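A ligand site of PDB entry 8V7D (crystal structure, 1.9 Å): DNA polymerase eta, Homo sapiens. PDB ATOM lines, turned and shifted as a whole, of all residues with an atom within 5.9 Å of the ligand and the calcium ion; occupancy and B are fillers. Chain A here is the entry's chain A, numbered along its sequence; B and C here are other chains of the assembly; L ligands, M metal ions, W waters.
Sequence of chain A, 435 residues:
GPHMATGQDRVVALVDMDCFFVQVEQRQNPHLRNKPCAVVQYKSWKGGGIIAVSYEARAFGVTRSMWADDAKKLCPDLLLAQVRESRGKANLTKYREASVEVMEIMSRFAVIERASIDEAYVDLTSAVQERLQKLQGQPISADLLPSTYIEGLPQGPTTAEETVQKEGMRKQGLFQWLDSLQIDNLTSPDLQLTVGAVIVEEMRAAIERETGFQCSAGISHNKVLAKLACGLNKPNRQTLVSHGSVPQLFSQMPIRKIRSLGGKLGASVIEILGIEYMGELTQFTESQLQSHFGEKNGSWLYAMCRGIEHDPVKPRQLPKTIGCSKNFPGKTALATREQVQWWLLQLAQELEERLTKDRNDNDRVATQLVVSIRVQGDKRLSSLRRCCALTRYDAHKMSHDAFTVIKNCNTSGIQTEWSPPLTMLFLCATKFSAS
The calcium ion is bound by OD1 of Asp 16, 2.2 Å away. The calcium ion is bound by an oxygen (O9) of the ligand, at 2.2 Å. OD2 of Asp 118 is bound to the calcium ion, 2.2 Å away. The calcium ion is bound by O12 of the ligand. The backbone carbonyl oxygen (O) of Met 17 is bound to the calcium ion, at 2.3 Å. The calcium ion is bound by an oxygen (O6) of the ligand, at 2.3 Å.
Water W2 lies within hydrogen-bond range of O4 of the ligand, N of Phe 21 and N of Phe 20. Water W3 lies within hydrogen-bond range of O10 of the ligand (2.8 Å), N of Val 53 (2.9 Å) and NH2 of Arg 58 (3.0 Å).
NH1 of Arg 58 sits close to OH of Tyr 55 (3.2 Å). O3' of DT 8 of chain C lies within hydrogen-bond range of OG of Ser 116, at 2.6 Å. The guanidinium group (NE) of Arg 58 is in hydrogen-bond range of the backbone carbonyl oxygen (O) of Val 53 (2.9 Å). The backbone carbonyl oxygen (O) of Asp 16 lies within hydrogen-bond range of the side-chain amino group (NZ) of Lys 234, 3.5 Å away. N of Asp 118 lies close to OG of Ser 116 (3.1 Å). The guanidinium group of Arg 64 sits at hydrogen-bond distance from the backbone carbonyl oxygen of Ile 51, at 2.6 Å. The side-chain carboxylate (OD1) of Asp 18 is in salt-bridge range of the side-chain amino group (NZ) of Lys 234, at 3.0 Å.
An oxygen (O14) of the ligand is in hydrogen-bond range of the backbone NH (N) of Cys 19 (2.9 Å). NH1 of Arg 64 is in salt-bridge range of O7 of the ligand, at 3.0 Å. An oxygen (O14) of the ligand is in salt-bridge range of the side-chain amino group of Lys 234 (3.6 Å). An oxygen (O14) of the ligand lies within hydrogen-bond range of the side-chain hydroxyl of Tyr 55. O6 of DG 4 of chain B sits at hydrogen-bond distance from a nitrogen (N3) of the ligand, 3.2 Å away. An oxygen (O9) of the ligand sits close to the backbone NH (N) of Phe 20 (3.3 Å). O14 of the ligand lies within salt-bridge range of NH2 of Arg 58, 3.3 Å away.
Within 4 Å of the calcium ion: Asp 16, Met 17 and Asp 118. The nearest printed residue that does not touch the calcium ion is Lys 234 (4.3 Å).
O1 of the ligand sits close to N1 of DA 5 of chain B. N3 of DT 8 of chain C sits close to a nitrogen (N2) of the ligand, at 3.3 Å. Asp 18 touches the ligand (CA to O14, 3.4 Å). CZ of Phe 21 touches O2 of the ligand (3.0 Å). Ala 52 touches the ligand. Ile 117 touches the ligand. DT 3 of chain B touches the ligand. The nearest printed residue that does not touch the ligand is Ile 51 (4.6 Å).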
ATOM      1  N   ASP A  16      -7.931   1.768  10.407  1.00  0.00           N
ATOM      2  CA  ASP A  16      -9.322   1.317  10.259  1.00  0.00           C
ATOM      3  C   ASP A  16      -9.422   0.459   8.997  1.00  0.00           C
ATOM      4  O   ASP A  16      -9.202   0.967   7.903  1.00  0.00           O
ATOM      5  CB  ASP A  16     -10.251   2.508  10.095  1.00  0.00           C
ATOM      6  CG  ASP A  16     -11.731   2.203  10.265  1.00  0.00           C
ATOM      7  OD1 ASP A  16     -12.135   1.089   9.911  1.00  0.00           O
ATOM      8  OD2 ASP A  16     -12.444   3.093  10.745  1.00  0.00           O
ATOM      9  N   MET A  17      -9.831  -0.807   9.149  1.00  0.00           N
ATOM     10  CA  MET A  17      -9.996  -1.711   8.007  1.00  0.00           C
ATOM     11  C   MET A  17     -11.133  -1.185   7.138  1.00  0.00           C
ATOM     12  O   MET A  17     -12.205  -0.856   7.649  1.00  0.00           O
ATOM     13  CB  MET A  17     -10.354  -3.097   8.529  1.00  0.00           C
ATOM     14  CG  MET A  17      -9.271  -3.805   9.322  1.00  0.00           C
ATOM     15  SD  MET A  17      -7.581  -3.477   8.855  1.00  0.00           S
ATOM     16  CE  MET A  17      -7.389  -4.565   7.483  1.00  0.00           C
ATOM     17  N   ASP A  18     -10.895  -1.052   5.829  1.00  0.00           N
ATOM     18  CA  ASP A  18     -11.967  -0.685   4.864  1.00  0.00           C
ATOM     19  C   ASP A  18     -13.002  -1.817   4.719  1.00  0.00           C
ATOM     20  O   ASP A  18     -12.526  -2.955   4.601  1.00  0.00           O
ATOM     21  CB  ASP A  18     -11.351  -0.366   3.502  1.00  0.00           C
ATOM     22  CG  ASP A  18     -10.330   0.757   3.536  1.00  0.00           C
ATOM     23  OD1 ASP A  18     -10.574   1.746   4.242  1.00  0.00           O
ATOM     24  OD2 ASP A  18      -9.305   0.636   2.853  1.00  0.00           O
ATOM     25  N   CYS A  19     -14.311  -1.503   4.694  1.00  0.00           N
ATOM     26  CA  CYS A  19     -15.447  -2.467   4.550  1.00  0.00           C
ATOM     27  C   CYS A  19     -15.032  -3.830   5.108  1.00  0.00           C
ATOM     28  O   CYS A  19     -15.032  -4.795   4.357  1.00  0.00           O
ATOM     29  CB  CYS A  19     -15.952  -2.516   3.111  1.00  0.00           C
ATOM     30  SG  CYS A  19     -14.679  -2.700   1.837  1.00  0.00           S
ATOM     31  N   PHE A  20     -14.645  -3.850   6.375  1.00  0.00           N
ATOM     32  CA  PHE A  20     -13.988  -5.038   6.968  1.00  0.00           C
ATOM     33  C   PHE A  20     -14.715  -6.345   6.672  1.00  0.00           C
ATOM     34  O   PHE A  20     -14.071  -7.219   6.087  1.00  0.00           O
ATOM     35  CB  PHE A  20     -13.783  -4.902   8.466  1.00  0.00           C
ATOM     36  CG  PHE A  20     -12.912  -5.979   9.049  1.00  0.00           C
ATOM     37  CD1 PHE A  20     -11.758  -6.367   8.399  1.00  0.00           C
ATOM     38  CD2 PHE A  20     -13.270  -6.635  10.209  1.00  0.00           C
ATOM     39  CE1 PHE A  20     -10.952  -7.373   8.922  1.00  0.00           C
ATOM     40  CE2 PHE A  20     -12.470  -7.636  10.725  1.00  0.00           C
ATOM     41  CZ  PHE A  20     -11.315  -8.006  10.084  1.00  0.00           C
ATOM     42  N   PHE A  21     -15.992  -6.497   7.076  1.00  0.00           N
ATOM     43  CA  PHE A  21     -16.618  -7.798   6.901  1.00  0.00           C
ATOM     44  C   PHE A  21     -16.699  -8.172   5.426  1.00  0.00           C
ATOM     45  O   PHE A  21     -16.605  -9.369   5.057  1.00  0.00           O
ATOM     46  CB  PHE A  21     -18.019  -7.849   7.524  1.00  0.00           C
ATOM     47  CG  PHE A  21     -18.065  -7.832   9.032  1.00  0.00           C
ATOM     48  CD1 PHE A  21     -16.989  -7.486   9.804  1.00  0.00           C
ATOM     49  CD2 PHE A  21     -19.233  -8.235   9.659  1.00  0.00           C
ATOM     50  CE1 PHE A  21     -17.080  -7.489  11.206  1.00  0.00           C
ATOM     51  CE2 PHE A  21     -19.338  -8.239  11.043  1.00  0.00           C
ATOM     52  CZ  PHE A  21     -18.258  -7.869  11.812  1.00  0.00           C
ATOM     53  N   ILE A  51     -24.991  -5.195   7.248  1.00  0.00           N
ATOM     54  CA  ILE A  51     -24.069  -4.654   8.235  1.00  0.00           C
ATOM     55  C   ILE A  51     -22.798  -4.103   7.634  1.00  0.00           C
ATOM     56  O   ILE A  51     -22.077  -3.388   8.347  1.00  0.00           O
ATOM     57  CB  ILE A  51     -23.730  -5.707   9.319  1.00  0.00           C
ATOM     58  CG1 ILE A  51     -23.100  -6.933   8.696  1.00  0.00           C
ATOM     59  CG2 ILE A  51     -25.018  -6.149  10.062  1.00  0.00           C
ATOM     60  CD1 ILE A  51     -23.196  -8.134   9.596  1.00  0.00           C
ATOM     61  N   ALA A  52     -22.482  -4.387   6.371  1.00  0.00           N
ATOM     62  CA  ALA A  52     -21.259  -3.891   5.751  1.00  0.00           C
ATOM     63  C   ALA A  52     -21.432  -3.892   4.230  1.00  0.00           C
ATOM     64  O   ALA A  52     -22.152  -4.725   3.698  1.00  0.00           O
ATOM     65  CB  ALA A  52     -20.029  -4.728   6.138  1.00  0.00           C
ATOM     66  N   VAL A  53     -20.776  -2.933   3.562  1.00  0.00           N
ATOM     67  CA  VAL A  53     -21.080  -2.613   2.164  1.00  0.00           C
ATOM     68  C   VAL A  53     -19.781  -2.316   1.413  1.00  0.00           C
ATOM     69  O   VAL A  53     -19.006  -1.446   1.844  1.00  0.00           O
ATOM     70  CB  VAL A  53     -22.032  -1.407   2.061  1.00  0.00           C
ATOM     71  CG1 VAL A  53     -22.515  -1.221   0.626  1.00  0.00           C
ATOM     72  CG2 VAL A  53     -23.210  -1.557   2.984  1.00  0.00           C
ATOM     73  N   TYR A  55     -17.377  -0.725  -1.519  1.00  0.00           N
ATOM     74  CA  TYR A  55     -17.414   0.632  -2.069  1.00  0.00           C
ATOM     75  C   TYR A  55     -18.181   0.672  -3.393  1.00  0.00           C
ATOM     76  O   TYR A  55     -18.908   1.640  -3.684  1.00  0.00           O
ATOM     77  CB  TYR A  55     -15.972   1.180  -2.177  1.00  0.00           C
ATOM     78  CG  TYR A  55     -15.526   1.717  -0.816  1.00  0.00           C
ATOM     79  CD1 TYR A  55     -15.144   0.836   0.169  1.00  0.00           C
ATOM     80  CD2 TYR A  55     -15.560   3.079  -0.491  1.00  0.00           C
ATOM     81  CE1 TYR A  55     -14.756   1.265   1.442  1.00  0.00           C
ATOM     82  CE2 TYR A  55     -15.178   3.532   0.802  1.00  0.00           C
ATOM     83  CZ  TYR A  55     -14.793   2.603   1.770  1.00  0.00           C
ATOM     84  OH  TYR A  55     -14.395   2.963   3.066  1.00  0.00           O
ATOM     85  N   ARG A  58     -21.760   0.908  -2.374  1.00  0.00           N
ATOM     86  CA  ARG A  58     -22.066   2.227  -1.812  1.00  0.00           C
ATOM     87  C   ARG A  58     -22.344   3.251  -2.894  1.00  0.00           C
ATOM     88  O   ARG A  58     -23.094   4.217  -2.661  1.00  0.00           O
ATOM     89  CB  ARG A  58     -20.926   2.731  -0.942  1.00  0.00           C
ATOM     90  CG  ARG A  58     -20.616   1.827   0.229  1.00  0.00           C
ATOM     91  CD  ARG A  58     -19.407   2.353   0.959  1.00  0.00           C
ATOM     92  NE  ARG A  58     -18.881   1.403   1.920  1.00  0.00           N
ATOM     93  CZ  ARG A  58     -18.064   1.739   2.908  1.00  0.00           C
ATOM     94  NH1 ARG A  58     -17.644   2.984   3.075  1.00  0.00           N
ATOM     95  NH2 ARG A  58     -17.667   0.798   3.768  1.00  0.00           N
ATOM     96  N   ARG A  64     -25.262   0.462   5.477  1.00  0.00           N
ATOM     97  CA  ARG A  64     -25.498  -0.263   6.705  1.00  0.00           C
ATOM     98  C   ARG A  64     -26.899   0.026   7.240  1.00  0.00           C
ATOM     99  O   ARG A  64     -27.430   1.129   7.045  1.00  0.00           O
ATOM    100  CB  ARG A  64     -24.440   0.141   7.737  1.00  0.00           C
ATOM    101  CG  ARG A  64     -24.586  -0.414   9.121  1.00  0.00           C
ATOM    102  CD  ARG A  64     -23.312  -0.098   9.873  1.00  0.00           C
ATOM    103  NE  ARG A  64     -22.248  -0.943   9.352  1.00  0.00           N
ATOM    104  CZ  ARG A  64     -20.968  -0.621   9.315  1.00  0.00           C
ATOM    105  NH1 ARG A  64     -20.537   0.569   9.735  1.00  0.00           N
ATOM    106  NH2 ARG A  64     -20.101  -1.490   8.812  1.00  0.00           N
ATOM    107  N   LEU A  92     -20.134 -14.025  15.061  1.00  0.00           N
ATOM    108  CA  LEU A  92     -19.164 -13.198  14.352  1.00  0.00           C
ATOM    109  C   LEU A  92     -17.763 -13.767  14.435  1.00  0.00           C
ATOM    110  O   LEU A  92     -16.797 -13.017  14.262  1.00  0.00           O
ATOM    111  CB  LEU A  92     -19.187 -11.782  14.939  1.00  0.00           C
ATOM    112  CG  LEU A  92     -20.590 -11.172  14.972  1.00  0.00           C
ATOM    113  CD1 LEU A  92     -20.568  -9.833  15.677  1.00  0.00           C
ATOM    114  CD2 LEU A  92     -21.047 -10.996  13.552  1.00  0.00           C
ATOM    115  N   SER A 116     -11.879  -1.313  18.263  1.00  0.00           N
ATOM    116  CA  SER A 116     -13.102  -2.037  17.870  1.00  0.00           C
ATOM    117  C   SER A 116     -12.654  -3.318  17.187  1.00  0.00           C
ATOM    118  O   SER A 116     -11.453  -3.566  17.127  1.00  0.00           O
ATOM    119  CB  SER A 116     -13.910  -1.215  16.941  1.00  0.00           C
ATOM    120  OG  SER A 116     -13.290  -1.144  15.661  1.00  0.00           O
ATOM    121  N   ILE A 117     -13.613  -4.063  16.659  1.00  0.00           N
ATOM    122  CA  ILE A 117     -13.219  -5.247  15.889  1.00  0.00           C
ATOM    123  C   ILE A 117     -12.238  -4.900  14.776  1.00  0.00           C
ATOM    124  O   ILE A 117     -11.370  -5.727  14.430  1.00  0.00           O
ATOM    125  CB  ILE A 117     -14.447  -5.994  15.324  1.00  0.00           C
ATOM    126  CG1 ILE A 117     -14.006  -7.361  14.787  1.00  0.00           C
ATOM    127  CG2 ILE A 117     -15.130  -5.177  14.233  1.00  0.00           C
ATOM    128  CD1 ILE A 117     -15.160  -8.389  14.680  1.00  0.00           C
ATOM    129  N   ASP A 118     -12.314  -3.686  14.203  1.00  0.00           N
ATOM    130  CA  ASP A 118     -11.497  -3.425  13.023  1.00  0.00           C
ATOM    131  C   ASP A 118     -10.724  -2.107  13.076  1.00  0.00           C
ATOM    132  O   ASP A 118     -10.267  -1.624  12.033  1.00  0.00           O
ATOM    133  CB  ASP A 118     -12.358  -3.476  11.760  1.00  0.00           C
ATOM    134  CG  ASP A 118     -13.100  -2.205  11.518  1.00  0.00           C
ATOM    135  OD1 ASP A 118     -13.449  -1.535  12.526  1.00  0.00           O
ATOM    136  OD2 ASP A 118     -13.319  -1.883  10.340  1.00  0.00           O
ATOM    137  N   GLU A 119     -10.539  -1.521  14.258  1.00  0.00           N
ATOM    138  CA  GLU A 119      -9.765  -0.288  14.450  1.00  0.00           C
ATOM    139  C   GLU A 119      -8.798  -0.474  15.607  1.00  0.00           C
ATOM    140  O   GLU A 119      -9.183  -1.077  16.630  1.00  0.00           O
ATOM    141  CB  GLU A 119     -10.691   0.872  14.799  1.00  0.00           C
ATOM    142  CG  GLU A 119     -11.397   1.530  13.647  1.00  0.00           C
ATOM    143  CD  GLU A 119     -12.229   2.709  14.115  1.00  0.00           C
ATOM    144  OE1 GLU A 119     -11.875   3.302  15.147  1.00  0.00           O
ATOM    145  OE2 GLU A 119     -13.236   3.022  13.458  1.00  0.00           O
ATOM    146  N   LYS A 234     -10.543   7.790   2.133  1.00  0.00           N
ATOM    147  CA  LYS A 234     -10.881   6.384   2.239  1.00  0.00           C
ATOM    148  C   LYS A 234     -11.355   5.948   0.863  1.00  0.00           C
ATOM    149  O   LYS A 234     -11.792   6.791   0.067  1.00  0.00           O
ATOM    150  CB  LYS A 234     -11.989   6.183   3.290  1.00  0.00           C
ATOM    151  CG  LYS A 234     -11.553   5.575   4.630  1.00  0.00           C
ATOM    152  CD  LYS A 234     -12.753   5.016   5.429  1.00  0.00           C
ATOM    153  CE  LYS A 234     -12.380   4.302   6.747  1.00  0.00           C
ATOM    154  NZ  LYS A 234     -11.875   2.840   6.659  1.00  0.00           N
ATOM    155  N   PRO A 235     -11.211   4.659   0.510  1.00  0.00           N
ATOM    156  CA  PRO A 235     -10.504   3.565   1.174  1.00  0.00           C
ATOM    157  C   PRO A 235      -9.037   3.512   0.738  1.00  0.00           C
ATOM    158  O   PRO A 235      -8.670   4.182  -0.214  1.00  0.00           O
ATOM    159  CB  PRO A 235     -11.257   2.330   0.679  1.00  0.00           C
ATOM    160  CG  PRO A 235     -11.597   2.695  -0.733  1.00  0.00           C
ATOM    161  CD  PRO A 235     -11.877   4.190  -0.726  1.00  0.00           C
ATOM    162  P    DT B   3     -36.770  -0.855  12.177  1.00  0.00           P
ATOM    163  OP1  DT B   3     -37.852  -0.043  12.782  1.00  0.00           O
ATOM    164  OP2  DT B   3     -36.234  -0.528  10.833  1.00  0.00           O
ATOM    165  O5'  DT B   3     -35.539  -0.838  13.202  1.00  0.00           O
ATOM    166  C5'  DT B   3     -34.215  -0.919  12.716  1.00  0.00           C
ATOM    167  C4'  DT B   3     -33.752  -2.355  12.651  1.00  0.00           C
ATOM    168  O4'  DT B   3     -32.484  -2.433  11.951  1.00  0.00           O
ATOM    169  C3'  DT B   3     -33.525  -3.025  13.995  1.00  0.00           C
ATOM    170  O3'  DT B   3     -33.864  -4.381  13.895  1.00  0.00           O
ATOM    171  C2'  DT B   3     -32.023  -2.843  14.205  1.00  0.00           C
ATOM    172  C1'  DT B   3     -31.518  -3.028  12.786  1.00  0.00           C
ATOM    173  N1   DT B   3     -30.198  -2.355  12.526  1.00  0.00           N
ATOM    174  C2   DT B   3     -29.174  -3.062  11.902  1.00  0.00           C
ATOM    175  O2   DT B   3     -29.284  -4.226  11.547  1.00  0.00           O
ATOM    176  N3   DT B   3     -28.012  -2.349  11.722  1.00  0.00           N
ATOM    177  C4   DT B   3     -27.772  -1.016  12.077  1.00  0.00           C
ATOM    178  O4   DT B   3     -26.692  -0.458  11.862  1.00  0.00           O
ATOM    179  C5   DT B   3     -28.903  -0.342  12.717  1.00  0.00           C
ATOM    180  C7   DT B   3     -28.785   1.093  13.157  1.00  0.00           C
ATOM    181  C6   DT B   3     -30.035  -1.042  12.909  1.00  0.00           C
ATOM    182  P    DG B   4     -33.683  -5.357  15.140  1.00  0.00           P
ATOM    183  OP1  DG B   4     -34.573  -6.503  14.824  1.00  0.00           O
ATOM    184  OP2  DG B   4     -33.739  -4.601  16.408  1.00  0.00           O
ATOM    185  O5'  DG B   4     -32.184  -5.878  15.029  1.00  0.00           O
ATOM    186  C5'  DG B   4     -31.806  -6.781  13.985  1.00  0.00           C
ATOM    187  C4'  DG B   4     -30.421  -7.287  14.298  1.00  0.00           C
ATOM    188  O4'  DG B   4     -29.475  -6.220  14.085  1.00  0.00           O
ATOM    189  C3'  DG B   4     -30.214  -7.725  15.743  1.00  0.00           C
ATOM    190  O3'  DG B   4     -29.189  -8.700  15.758  1.00  0.00           O
ATOM    191  C2'  DG B   4     -29.722  -6.442  16.387  1.00  0.00           C
ATOM    192  C1'  DG B   4     -28.785  -5.969  15.300  1.00  0.00           C
ATOM    193  N9   DG B   4     -28.450  -4.551  15.368  1.00  0.00           N
ATOM    194  C8   DG B   4     -29.219  -3.462  15.693  1.00  0.00           C
ATOM    195  N7   DG B   4     -28.549  -2.336  15.633  1.00  0.00           N
ATOM    196  C5   DG B   4     -27.276  -2.708  15.256  1.00  0.00           C
ATOM    197  C6   DG B   4     -26.117  -1.925  15.030  1.00  0.00           C
ATOM    198  O6   DG B   4     -25.995  -0.698  15.131  1.00  0.00           O
ATOM    199  N1   DG B   4     -25.034  -2.714  14.661  1.00  0.00           N
ATOM    200  C2   DG B   4     -25.058  -4.086  14.515  1.00  0.00           C
ATOM    201  N2   DG B   4     -23.915  -4.679  14.150  1.00  0.00           N
ATOM    202  N3   DG B   4     -26.139  -4.823  14.726  1.00  0.00           N
ATOM    203  C4   DG B   4     -27.204  -4.075  15.085  1.00  0.00           C
ATOM    204  P    DA B   5     -28.723  -9.382  17.129  1.00  0.00           P
ATOM    205  OP1  DA B   5     -28.784 -10.847  16.842  1.00  0.00           O
ATOM    206  OP2  DA B   5     -29.464  -8.852  18.276  1.00  0.00           O
ATOM    207  O5'  DA B   5     -27.194  -8.998  17.230  1.00  0.00           O
ATOM    208  C5'  DA B   5     -26.299  -9.461  16.250  1.00  0.00           C
ATOM    209  C4'  DA B   5     -24.894  -9.283  16.724  1.00  0.00           C
ATOM    210  O4'  DA B   5     -24.523  -7.870  16.666  1.00  0.00           O
ATOM    211  C3'  DA B   5     -24.643  -9.719  18.159  1.00  0.00           C
ATOM    212  O3'  DA B   5     -23.339 -10.258  18.244  1.00  0.00           O
ATOM    213  C2'  DA B   5     -24.787  -8.406  18.941  1.00  0.00           C
ATOM    214  C1'  DA B   5     -24.175  -7.418  17.945  1.00  0.00           C
ATOM    215  N9   DA B   5     -24.650  -6.038  18.076  1.00  0.00           N
ATOM    216  C8   DA B   5     -25.924  -5.590  18.308  1.00  0.00           C
ATOM    217  N7   DA B   5     -26.028  -4.265  18.349  1.00  0.00           N
ATOM    218  C5   DA B   5     -24.733  -3.821  18.120  1.00  0.00           C
ATOM    219  C6   DA B   5     -24.155  -2.545  18.028  1.00  0.00           C
ATOM    220  N6   DA B   5     -24.850  -1.413  18.194  1.00  0.00           N
ATOM    221  N1   DA B   5     -22.833  -2.458  17.780  1.00  0.00           N
ATOM    222  C2   DA B   5     -22.131  -3.585  17.626  1.00  0.00           C
ATOM    223  N3   DA B   5     -22.562  -4.853  17.678  1.00  0.00           N
ATOM    224  C4   DA B   5     -23.872  -4.895  17.943  1.00  0.00           C
ATOM    225  P    DT C   8     -16.154   5.608  16.595  1.00  0.00           P
ATOM    226  OP1  DT C   8     -15.349   5.540  17.838  1.00  0.00           O
ATOM    227  OP2  DT C   8     -15.662   6.348  15.424  1.00  0.00           O
ATOM    228  O5'  DT C   8     -16.428   4.103  16.123  1.00  0.00           O
ATOM    229  C5'  DT C   8     -15.495   3.150  16.458  1.00  0.00           C
ATOM    230  C4'  DT C   8     -15.924   1.732  16.105  1.00  0.00           C
ATOM    231  O4'  DT C   8     -17.147   1.301  16.750  1.00  0.00           O
ATOM    232  C3'  DT C   8     -16.006   1.308  14.660  1.00  0.00           C
ATOM    233  O3'  DT C   8     -15.111   0.204  14.448  1.00  0.00           O
ATOM    234  C2'  DT C   8     -17.478   0.923  14.463  1.00  0.00           C
ATOM    235  C1'  DT C   8     -17.869   0.489  15.876  1.00  0.00           C
ATOM    236  N1   DT C   8     -19.309   0.646  16.217  1.00  0.00           N
ATOM    237  C2   DT C   8     -19.964  -0.424  16.772  1.00  0.00           C
ATOM    238  O2   DT C   8     -19.429  -1.496  16.951  1.00  0.00           O
ATOM    239  N3   DT C   8     -21.272  -0.202  17.075  1.00  0.00           N
ATOM    240  C4   DT C   8     -21.977   0.960  16.927  1.00  0.00           C
ATOM    241  O4   DT C   8     -23.159   1.047  17.227  1.00  0.00           O
ATOM    242  C5   DT C   8     -21.237   2.060  16.343  1.00  0.00           C
ATOM    243  C7   DT C   8     -21.915   3.392  16.125  1.00  0.00           C
ATOM    244  C6   DT C   8     -19.947   1.860  16.024  1.00  0.00           C
HETATM  245  N1  LIG L   1     -20.351  -1.944  13.691  1.00  0.00           N
HETATM  246  C1  LIG L   1     -21.572  -2.295  14.250  1.00  0.00           C
HETATM  247  N2  LIG L   1     -22.596  -1.416  14.265  1.00  0.00           N
HETATM  248  C2  LIG L   1     -22.452  -0.198  13.732  1.00  0.00           C
HETATM  249  C3  LIG L   1     -21.212   0.182  13.159  1.00  0.00           C
HETATM  250  C4  LIG L   1     -20.187  -0.688  13.148  1.00  0.00           C
HETATM  251  O1  LIG L   1     -21.706  -3.409  14.733  1.00  0.00           O
HETATM  252  N3  LIG L   1     -23.476   0.638  13.765  1.00  0.00           N
HETATM  253  C5  LIG L   1     -19.265  -2.939  13.713  1.00  0.00           C
HETATM  254  C6  LIG L   1     -19.456  -3.971  12.606  1.00  0.00           C
HETATM  255  O2  LIG L   1     -18.933  -5.212  13.065  1.00  0.00           O
HETATM  256  C7  LIG L   1     -18.581  -3.444  11.490  1.00  0.00           C
HETATM  257  C8  LIG L   1     -17.388  -2.952  12.289  1.00  0.00           C
HETATM  258  O3  LIG L   1     -17.992  -2.346  13.462  1.00  0.00           O
HETATM  259  O4  LIG L   1     -18.205  -4.500  10.608  1.00  0.00           O
HETATM  260  C9  LIG L   1     -16.628  -1.905  11.520  1.00  0.00           C
HETATM  261  O5  LIG L   1     -17.480  -0.813  11.403  1.00  0.00           O
HETATM  262  P1  LIG L   1     -17.137   0.364  10.309  1.00  0.00           P
HETATM  263  O6  LIG L   1     -15.678   0.638  10.287  1.00  0.00           O
HETATM  264  O7  LIG L   1     -17.904   1.577  10.722  1.00  0.00           O
HETATM  265  O8  LIG L   1     -17.619  -0.107   8.873  1.00  0.00           O
HETATM  266  P2  LIG L   1     -16.769  -0.699   7.693  1.00  0.00           P
HETATM  267  O9  LIG L   1     -15.421  -1.200   8.132  1.00  0.00           O
HETATM  268  O10 LIG L   1     -17.565  -1.820   7.098  1.00  0.00           O
HETATM  269  O11 LIG L   1     -16.656   0.403   6.568  1.00  0.00           O
HETATM  270  P3  LIG L   1     -15.478   1.530   6.417  1.00  0.00           P
HETATM  271  O12 LIG L   1     -14.539   1.454   7.563  1.00  0.00           O
HETATM  272  O13 LIG L   1     -16.131   2.876   6.362  1.00  0.00           O
HETATM  273  O14 LIG L   1     -14.752   1.311   5.132  1.00  0.00           O
HETATM  274 CA    CA M   1     -13.785  -0.052   9.135  1.00  0.00          CA
HETATM  275  O   HOH W   1     -18.791   3.137   6.871  1.00  0.00           O
HETATM  276  O   HOH W   2     -17.472  -4.453   8.083  1.00  0.00           O
HETATM  277  O   HOH W   3     -19.524  -1.035   5.297  1.00  0.00           O
HETATM  278  O   HOH W   4     -23.630   3.304  12.901  1.00  0.00           O
HETATM  279  O   HOH W   5     -18.000  -4.821  15.762  1.00  0.00           O
